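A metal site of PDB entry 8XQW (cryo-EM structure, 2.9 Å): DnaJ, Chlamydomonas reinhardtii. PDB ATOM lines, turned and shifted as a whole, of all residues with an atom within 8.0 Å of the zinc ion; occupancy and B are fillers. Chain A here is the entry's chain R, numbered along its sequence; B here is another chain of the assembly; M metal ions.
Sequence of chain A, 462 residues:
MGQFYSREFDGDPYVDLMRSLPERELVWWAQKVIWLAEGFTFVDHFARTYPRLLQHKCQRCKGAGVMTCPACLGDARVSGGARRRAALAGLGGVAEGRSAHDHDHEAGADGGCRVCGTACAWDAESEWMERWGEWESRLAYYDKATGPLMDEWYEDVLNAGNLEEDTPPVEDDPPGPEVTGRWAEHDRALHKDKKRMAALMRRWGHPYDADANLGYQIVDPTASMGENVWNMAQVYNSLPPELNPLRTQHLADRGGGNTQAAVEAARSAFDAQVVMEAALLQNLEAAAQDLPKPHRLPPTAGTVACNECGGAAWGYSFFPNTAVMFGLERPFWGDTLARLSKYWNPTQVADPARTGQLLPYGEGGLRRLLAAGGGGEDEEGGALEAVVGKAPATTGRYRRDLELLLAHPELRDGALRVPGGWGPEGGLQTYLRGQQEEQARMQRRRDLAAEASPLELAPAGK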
ATOM      1  N   LYS A  57       2.652  -8.726   6.530  1.00  0.00           N
ATOM      2  CA  LYS A  57       2.780  -9.350   5.218  1.00  0.00           C
ATOM      3  C   LYS A  57       1.434  -9.863   4.735  1.00  0.00           C
ATOM      4  O   LYS A  57       0.551 -10.192   5.526  1.00  0.00           O
ATOM      5  CB  LYS A  57       3.757 -10.495   5.252  1.00  0.00           C
ATOM      6  CG  LYS A  57       5.164 -10.053   5.517  1.00  0.00           C
ATOM      7  CD  LYS A  57       6.112 -11.215   5.445  1.00  0.00           C
ATOM      8  CE  LYS A  57       5.499 -12.422   6.106  1.00  0.00           C
ATOM      9  NZ  LYS A  57       6.471 -13.527   6.256  1.00  0.00           N
ATOM     10  N   CYS A  58       1.281  -9.925   3.422  1.00  0.00           N
ATOM     11  CA  CYS A  58       0.077 -10.505   2.836  1.00  0.00           C
ATOM     12  C   CYS A  58      -0.017 -11.963   3.228  1.00  0.00           C
ATOM     13  O   CYS A  58       0.985 -12.678   3.232  1.00  0.00           O
ATOM     14  CB  CYS A  58       0.105 -10.360   1.319  1.00  0.00           C
ATOM     15  SG  CYS A  58      -1.367 -10.933   0.455  1.00  0.00           S
ATOM     16  N   GLN A  59      -1.213 -12.420   3.573  1.00  0.00           N
ATOM     17  CA  GLN A  59      -1.307 -13.780   4.072  1.00  0.00           C
ATOM     18  C   GLN A  59      -1.585 -14.787   2.974  1.00  0.00           C
ATOM     19  O   GLN A  59      -1.555 -15.985   3.251  1.00  0.00           O
ATOM     20  CB  GLN A  59      -2.396 -13.887   5.133  1.00  0.00           C
ATOM     21  CG  GLN A  59      -3.780 -13.653   4.629  1.00  0.00           C
ATOM     22  CD  GLN A  59      -4.815 -13.740   5.727  1.00  0.00           C
ATOM     23  OE1 GLN A  59      -4.801 -14.678   6.523  1.00  0.00           O
ATOM     24  NE2 GLN A  59      -5.710 -12.776   5.793  1.00  0.00           N
ATOM     25  N   ARG A  60      -1.842 -14.360   1.750  1.00  0.00           N
ATOM     26  CA  ARG A  60      -2.055 -15.315   0.680  1.00  0.00           C
ATOM     27  C   ARG A  60      -0.743 -15.707   0.008  1.00  0.00           C
ATOM     28  O   ARG A  60      -0.481 -16.896  -0.188  1.00  0.00           O
ATOM     29  CB  ARG A  60      -3.021 -14.758  -0.355  1.00  0.00           C
ATOM     30  CG  ARG A  60      -3.246 -15.729  -1.475  1.00  0.00           C
ATOM     31  CD  ARG A  60      -4.547 -15.519  -2.173  1.00  0.00           C
ATOM     32  NE  ARG A  60      -4.347 -15.313  -3.599  1.00  0.00           N
ATOM     33  CZ  ARG A  60      -4.055 -16.290  -4.460  1.00  0.00           C
ATOM     34  NH1 ARG A  60      -3.939 -17.542  -4.037  1.00  0.00           N
ATOM     35  NH2 ARG A  60      -3.884 -16.000  -5.750  1.00  0.00           N
ATOM     36  N   CYS A  61       0.068 -14.729  -0.354  1.00  0.00           N
ATOM     37  CA  CYS A  61       1.356 -15.000  -0.975  1.00  0.00           C
ATOM     38  C   CYS A  61       2.493 -15.091   0.027  1.00  0.00           C
ATOM     39  O   CYS A  61       3.611 -15.410  -0.369  1.00  0.00           O
ATOM     40  CB  CYS A  61       1.693 -13.924  -2.000  1.00  0.00           C
ATOM     41  SG  CYS A  61       1.369 -12.244  -1.482  1.00  0.00           S
ATOM     42  N   LYS A  62       2.231 -14.818   1.302  1.00  0.00           N
ATOM     43  CA  LYS A  62       3.247 -14.853   2.339  1.00  0.00           C
ATOM     44  C   LYS A  62       4.383 -13.879   2.034  1.00  0.00           C
ATOM     45  O   LYS A  62       5.546 -14.212   2.193  1.00  0.00           O
ATOM     46  CB  LYS A  62       3.797 -16.256   2.544  1.00  0.00           C
ATOM     47  CG  LYS A  62       2.727 -17.300   2.736  1.00  0.00           C
ATOM     48  CD  LYS A  62       3.312 -18.676   2.594  1.00  0.00           C
ATOM     49  CE  LYS A  62       2.277 -19.650   2.097  1.00  0.00           C
ATOM     50  NZ  LYS A  62       1.649 -19.169   0.839  1.00  0.00           N
ATOM     51  N   GLY A  63       4.032 -12.688   1.577  1.00  0.00           N
ATOM     52  CA  GLY A  63       5.015 -11.668   1.365  1.00  0.00           C
ATOM     53  C   GLY A  63       5.871 -11.824   0.138  1.00  0.00           C
ATOM     54  O   GLY A  63       6.897 -11.156   0.035  1.00  0.00           O
ATOM     55  N   ALA A  64       5.471 -12.683  -0.793  1.00  0.00           N
ATOM     56  CA  ALA A  64       6.186 -12.784  -2.057  1.00  0.00           C
ATOM     57  C   ALA A  64       5.626 -11.841  -3.101  1.00  0.00           C
ATOM     58  O   ALA A  64       6.353 -11.385  -3.983  1.00  0.00           O
ATOM     59  CB  ALA A  64       6.138 -14.216  -2.571  1.00  0.00           C
ATOM     60  N   GLY A  65       4.341 -11.521  -3.005  1.00  0.00           N
ATOM     61  CA  GLY A  65       3.710 -10.639  -3.958  1.00  0.00           C
ATOM     62  C   GLY A  65       3.450 -11.255  -5.311  1.00  0.00           C
ATOM     63  O   GLY A  65       3.158 -10.517  -6.250  1.00  0.00           O
ATOM     64  N   VAL A  66       3.531 -12.575  -5.429  1.00  0.00           N
ATOM     65  CA  VAL A  66       3.571 -13.240  -6.719  1.00  0.00           C
ATOM     66  C   VAL A  66       3.183 -14.697  -6.512  1.00  0.00           C
ATOM     67  O   VAL A  66       3.668 -15.348  -5.603  1.00  0.00           O
ATOM     68  CB  VAL A  66       4.977 -13.089  -7.355  1.00  0.00           C
ATOM     69  CG1 VAL A  66       5.347 -14.303  -8.107  1.00  0.00           C
ATOM     70  CG2 VAL A  66       5.009 -11.918  -8.280  1.00  0.00           C
ATOM     71  N   MET A  67       2.294 -15.191  -7.366  1.00  0.00           N
ATOM     72  CA  MET A  67       1.866 -16.579  -7.319  1.00  0.00           C
ATOM     73  C   MET A  67       2.246 -17.251  -8.631  1.00  0.00           C
ATOM     74  O   MET A  67       2.701 -16.600  -9.569  1.00  0.00           O
ATOM     75  CB  MET A  67       0.361 -16.667  -7.091  1.00  0.00           C
ATOM     76  CG  MET A  67      -0.112 -15.948  -5.848  1.00  0.00           C
ATOM     77  SD  MET A  67       0.553 -16.627  -4.318  1.00  0.00           S
ATOM     78  CE  MET A  67      -0.131 -18.272  -4.346  1.00  0.00           C
ATOM     79  N   ALA A 305       0.691 -11.994 -10.703  1.00  0.00           N
ATOM     80  CA  ALA A 305       0.661 -11.178  -9.504  1.00  0.00           C
ATOM     81  C   ALA A 305      -0.445 -11.637  -8.576  1.00  0.00           C
ATOM     82  O   ALA A 305      -1.507 -12.093  -9.010  1.00  0.00           O
ATOM     83  CB  ALA A 305       0.462  -9.717  -9.858  1.00  0.00           C
ATOM     84  N   CYS A 306      -0.201 -11.512  -7.281  1.00  0.00           N
ATOM     85  CA  CYS A 306      -1.203 -11.874  -6.293  1.00  0.00           C
ATOM     86  C   CYS A 306      -2.406 -10.943  -6.420  1.00  0.00           C
ATOM     87  O   CYS A 306      -2.248  -9.768  -6.763  1.00  0.00           O
ATOM     88  CB  CYS A 306      -0.620 -11.774  -4.890  1.00  0.00           C
ATOM     89  SG  CYS A 306      -1.704 -12.270  -3.571  1.00  0.00           S
ATOM     90  N   ASN A 307      -3.592 -11.469  -6.167  1.00  0.00           N
ATOM     91  CA  ASN A 307      -4.786 -10.654  -6.337  1.00  0.00           C
ATOM     92  C   ASN A 307      -5.420 -10.225  -5.030  1.00  0.00           C
ATOM     93  O   ASN A 307      -6.487  -9.612  -5.060  1.00  0.00           O
ATOM     94  CB  ASN A 307      -5.822 -11.395  -7.184  1.00  0.00           C
ATOM     95  CG  ASN A 307      -5.903 -12.845  -6.836  1.00  0.00           C
ATOM     96  OD1 ASN A 307      -4.968 -13.414  -6.282  1.00  0.00           O
ATOM     97  ND2 ASN A 307      -7.030 -13.464  -7.140  1.00  0.00           N
ATOM     98  N   GLU A 308      -4.810 -10.528  -3.889  1.00  0.00           N
ATOM     99  CA  GLU A 308      -5.243  -9.900  -2.649  1.00  0.00           C
ATOM    100  C   GLU A 308      -4.517  -8.587  -2.437  1.00  0.00           C
ATOM    101  O   GLU A 308      -5.149  -7.524  -2.420  1.00  0.00           O
ATOM    102  CB  GLU A 308      -4.996 -10.841  -1.482  1.00  0.00           C
ATOM    103  CG  GLU A 308      -5.607 -12.191  -1.687  1.00  0.00           C
ATOM    104  CD  GLU A 308      -7.073 -12.231  -1.292  1.00  0.00           C
ATOM    105  OE1 GLU A 308      -7.913 -12.626  -2.135  1.00  0.00           O
ATOM    106  OE2 GLU A 308      -7.390 -11.866  -0.142  1.00  0.00           O
ATOM    107  N   CYS A 309      -3.206  -8.628  -2.293  1.00  0.00           N
ATOM    108  CA  CYS A 309      -2.389  -7.455  -2.494  1.00  0.00           C
ATOM    109  C   CYS A 309      -2.324  -7.185  -3.988  1.00  0.00           C
ATOM    110  O   CYS A 309      -2.659  -8.042  -4.802  1.00  0.00           O
ATOM    111  CB  CYS A 309      -1.004  -7.659  -1.892  1.00  0.00           C
ATOM    112  SG  CYS A 309      -0.191  -9.174  -2.383  1.00  0.00           S
ATOM    113  N   GLY A 310      -1.893  -6.003  -4.372  1.00  0.00           N
ATOM    114  CA  GLY A 310      -1.746  -5.821  -5.794  1.00  0.00           C
ATOM    115  C   GLY A 310      -0.469  -6.362  -6.348  1.00  0.00           C
ATOM    116  O   GLY A 310      -0.180  -6.188  -7.535  1.00  0.00           O
ATOM    117  N   GLY A 311       0.315  -7.045  -5.523  1.00  0.00           N
ATOM    118  CA  GLY A 311       1.712  -7.266  -5.754  1.00  0.00           C
ATOM    119  C   GLY A 311       2.607  -6.529  -4.789  1.00  0.00           C
ATOM    120  O   GLY A 311       3.810  -6.787  -4.746  1.00  0.00           O
ATOM    121  N   ALA A 312       2.052  -5.591  -4.035  1.00  0.00           N
ATOM    122  CA  ALA A 312       2.747  -5.016  -2.900  1.00  0.00           C
ATOM    123  C   ALA A 312       2.726  -6.010  -1.768  1.00  0.00           C
ATOM    124  O   ALA A 312       1.675  -6.262  -1.175  1.00  0.00           O
ATOM    125  CB  ALA A 312       2.075  -3.724  -2.464  1.00  0.00           C
ATOM    126  N   ALA A 313       3.865  -6.594  -1.464  1.00  0.00           N
ATOM    127  CA  ALA A 313       3.865  -7.790  -0.655  1.00  0.00           C
ATOM    128  C   ALA A 313       3.587  -7.546   0.817  1.00  0.00           C
ATOM    129  O   ALA A 313       3.079  -8.449   1.488  1.00  0.00           O
ATOM    130  CB  ALA A 313       5.205  -8.509  -0.801  1.00  0.00           C
ATOM    131  N   TRP A 314       3.877  -6.366   1.336  1.00  0.00           N
ATOM    132  CA  TRP A 314       3.810  -6.128   2.773  1.00  0.00           C
ATOM    133  C   TRP A 314       3.564  -4.647   3.011  1.00  0.00           C
ATOM    134  O   TRP A 314       3.441  -3.870   2.071  1.00  0.00           O
ATOM    135  CB  TRP A 314       5.082  -6.605   3.442  1.00  0.00           C
ATOM    136  CG  TRP A 314       6.284  -5.977   2.889  1.00  0.00           C
ATOM    137  CD1 TRP A 314       6.951  -6.338   1.790  1.00  0.00           C
ATOM    138  CD2 TRP A 314       6.969  -4.845   3.420  1.00  0.00           C
ATOM    139  NE1 TRP A 314       8.023  -5.522   1.591  1.00  0.00           N
ATOM    140  CE2 TRP A 314       8.043  -4.590   2.583  1.00  0.00           C
ATOM    141  CE3 TRP A 314       6.775  -4.032   4.535  1.00  0.00           C
ATOM    142  CZ2 TRP A 314       8.925  -3.556   2.822  1.00  0.00           C
ATOM    143  CZ3 TRP A 314       7.629  -3.014   4.756  1.00  0.00           C
ATOM    144  CH2 TRP A 314       8.705  -2.775   3.908  1.00  0.00           C
ATOM    145  N   PHE B1362      -5.148  -4.055   2.916  1.00  0.00           N
ATOM    146  CA  PHE B1362      -5.307  -5.454   3.281  1.00  0.00           C
ATOM    147  C   PHE B1362      -4.827  -5.693   4.705  1.00  0.00           C
ATOM    148  O   PHE B1362      -5.394  -6.527   5.407  1.00  0.00           O
ATOM    149  CB  PHE B1362      -4.580  -6.362   2.291  1.00  0.00           C
ATOM    150  CG  PHE B1362      -3.136  -5.977   2.013  1.00  0.00           C
ATOM    151  CD1 PHE B1362      -2.832  -4.927   1.176  1.00  0.00           C
ATOM    152  CD2 PHE B1362      -2.095  -6.691   2.567  1.00  0.00           C
ATOM    153  CE1 PHE B1362      -1.517  -4.594   0.928  1.00  0.00           C
ATOM    154  CE2 PHE B1362      -0.802  -6.360   2.317  1.00  0.00           C
ATOM    155  CZ  PHE B1362      -0.508  -5.312   1.500  1.00  0.00           C
HETATM  156 ZN    ZN M   1      -0.532 -11.234  -1.729  1.00  0.00          ZN
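O of Ala 312 sits close to SG of Cys 309 (3.7 Å).
The backbone carbonyl oxygen (O) of Cys 58 lies within hydrogen-bond range of the backbone NH (N) of Gly 63, at 3.5 Å.
The side-chain sulfur (SG) of Cys 58 lies close to the backbone NH (N) of Arg 60 (3.7 Å).
The side-chain sulfur of Cys 306 lies close to the backbone NH of Glu 308 (3.6 Å).
The backbone carbonyl oxygen of Ala 313 lies within hydrogen-bond range of the backbone NH of Cys 58, 3.0 Å away.
The backbone NH (N) of Gly 65 sits close to the side-chain sulfur (SG) of Cys 61, at 3.4 Å.
The zinc ion is bound by SG of Cys 61, SG of Cys 309, SG of Cys 58 and SG of Cys 306.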
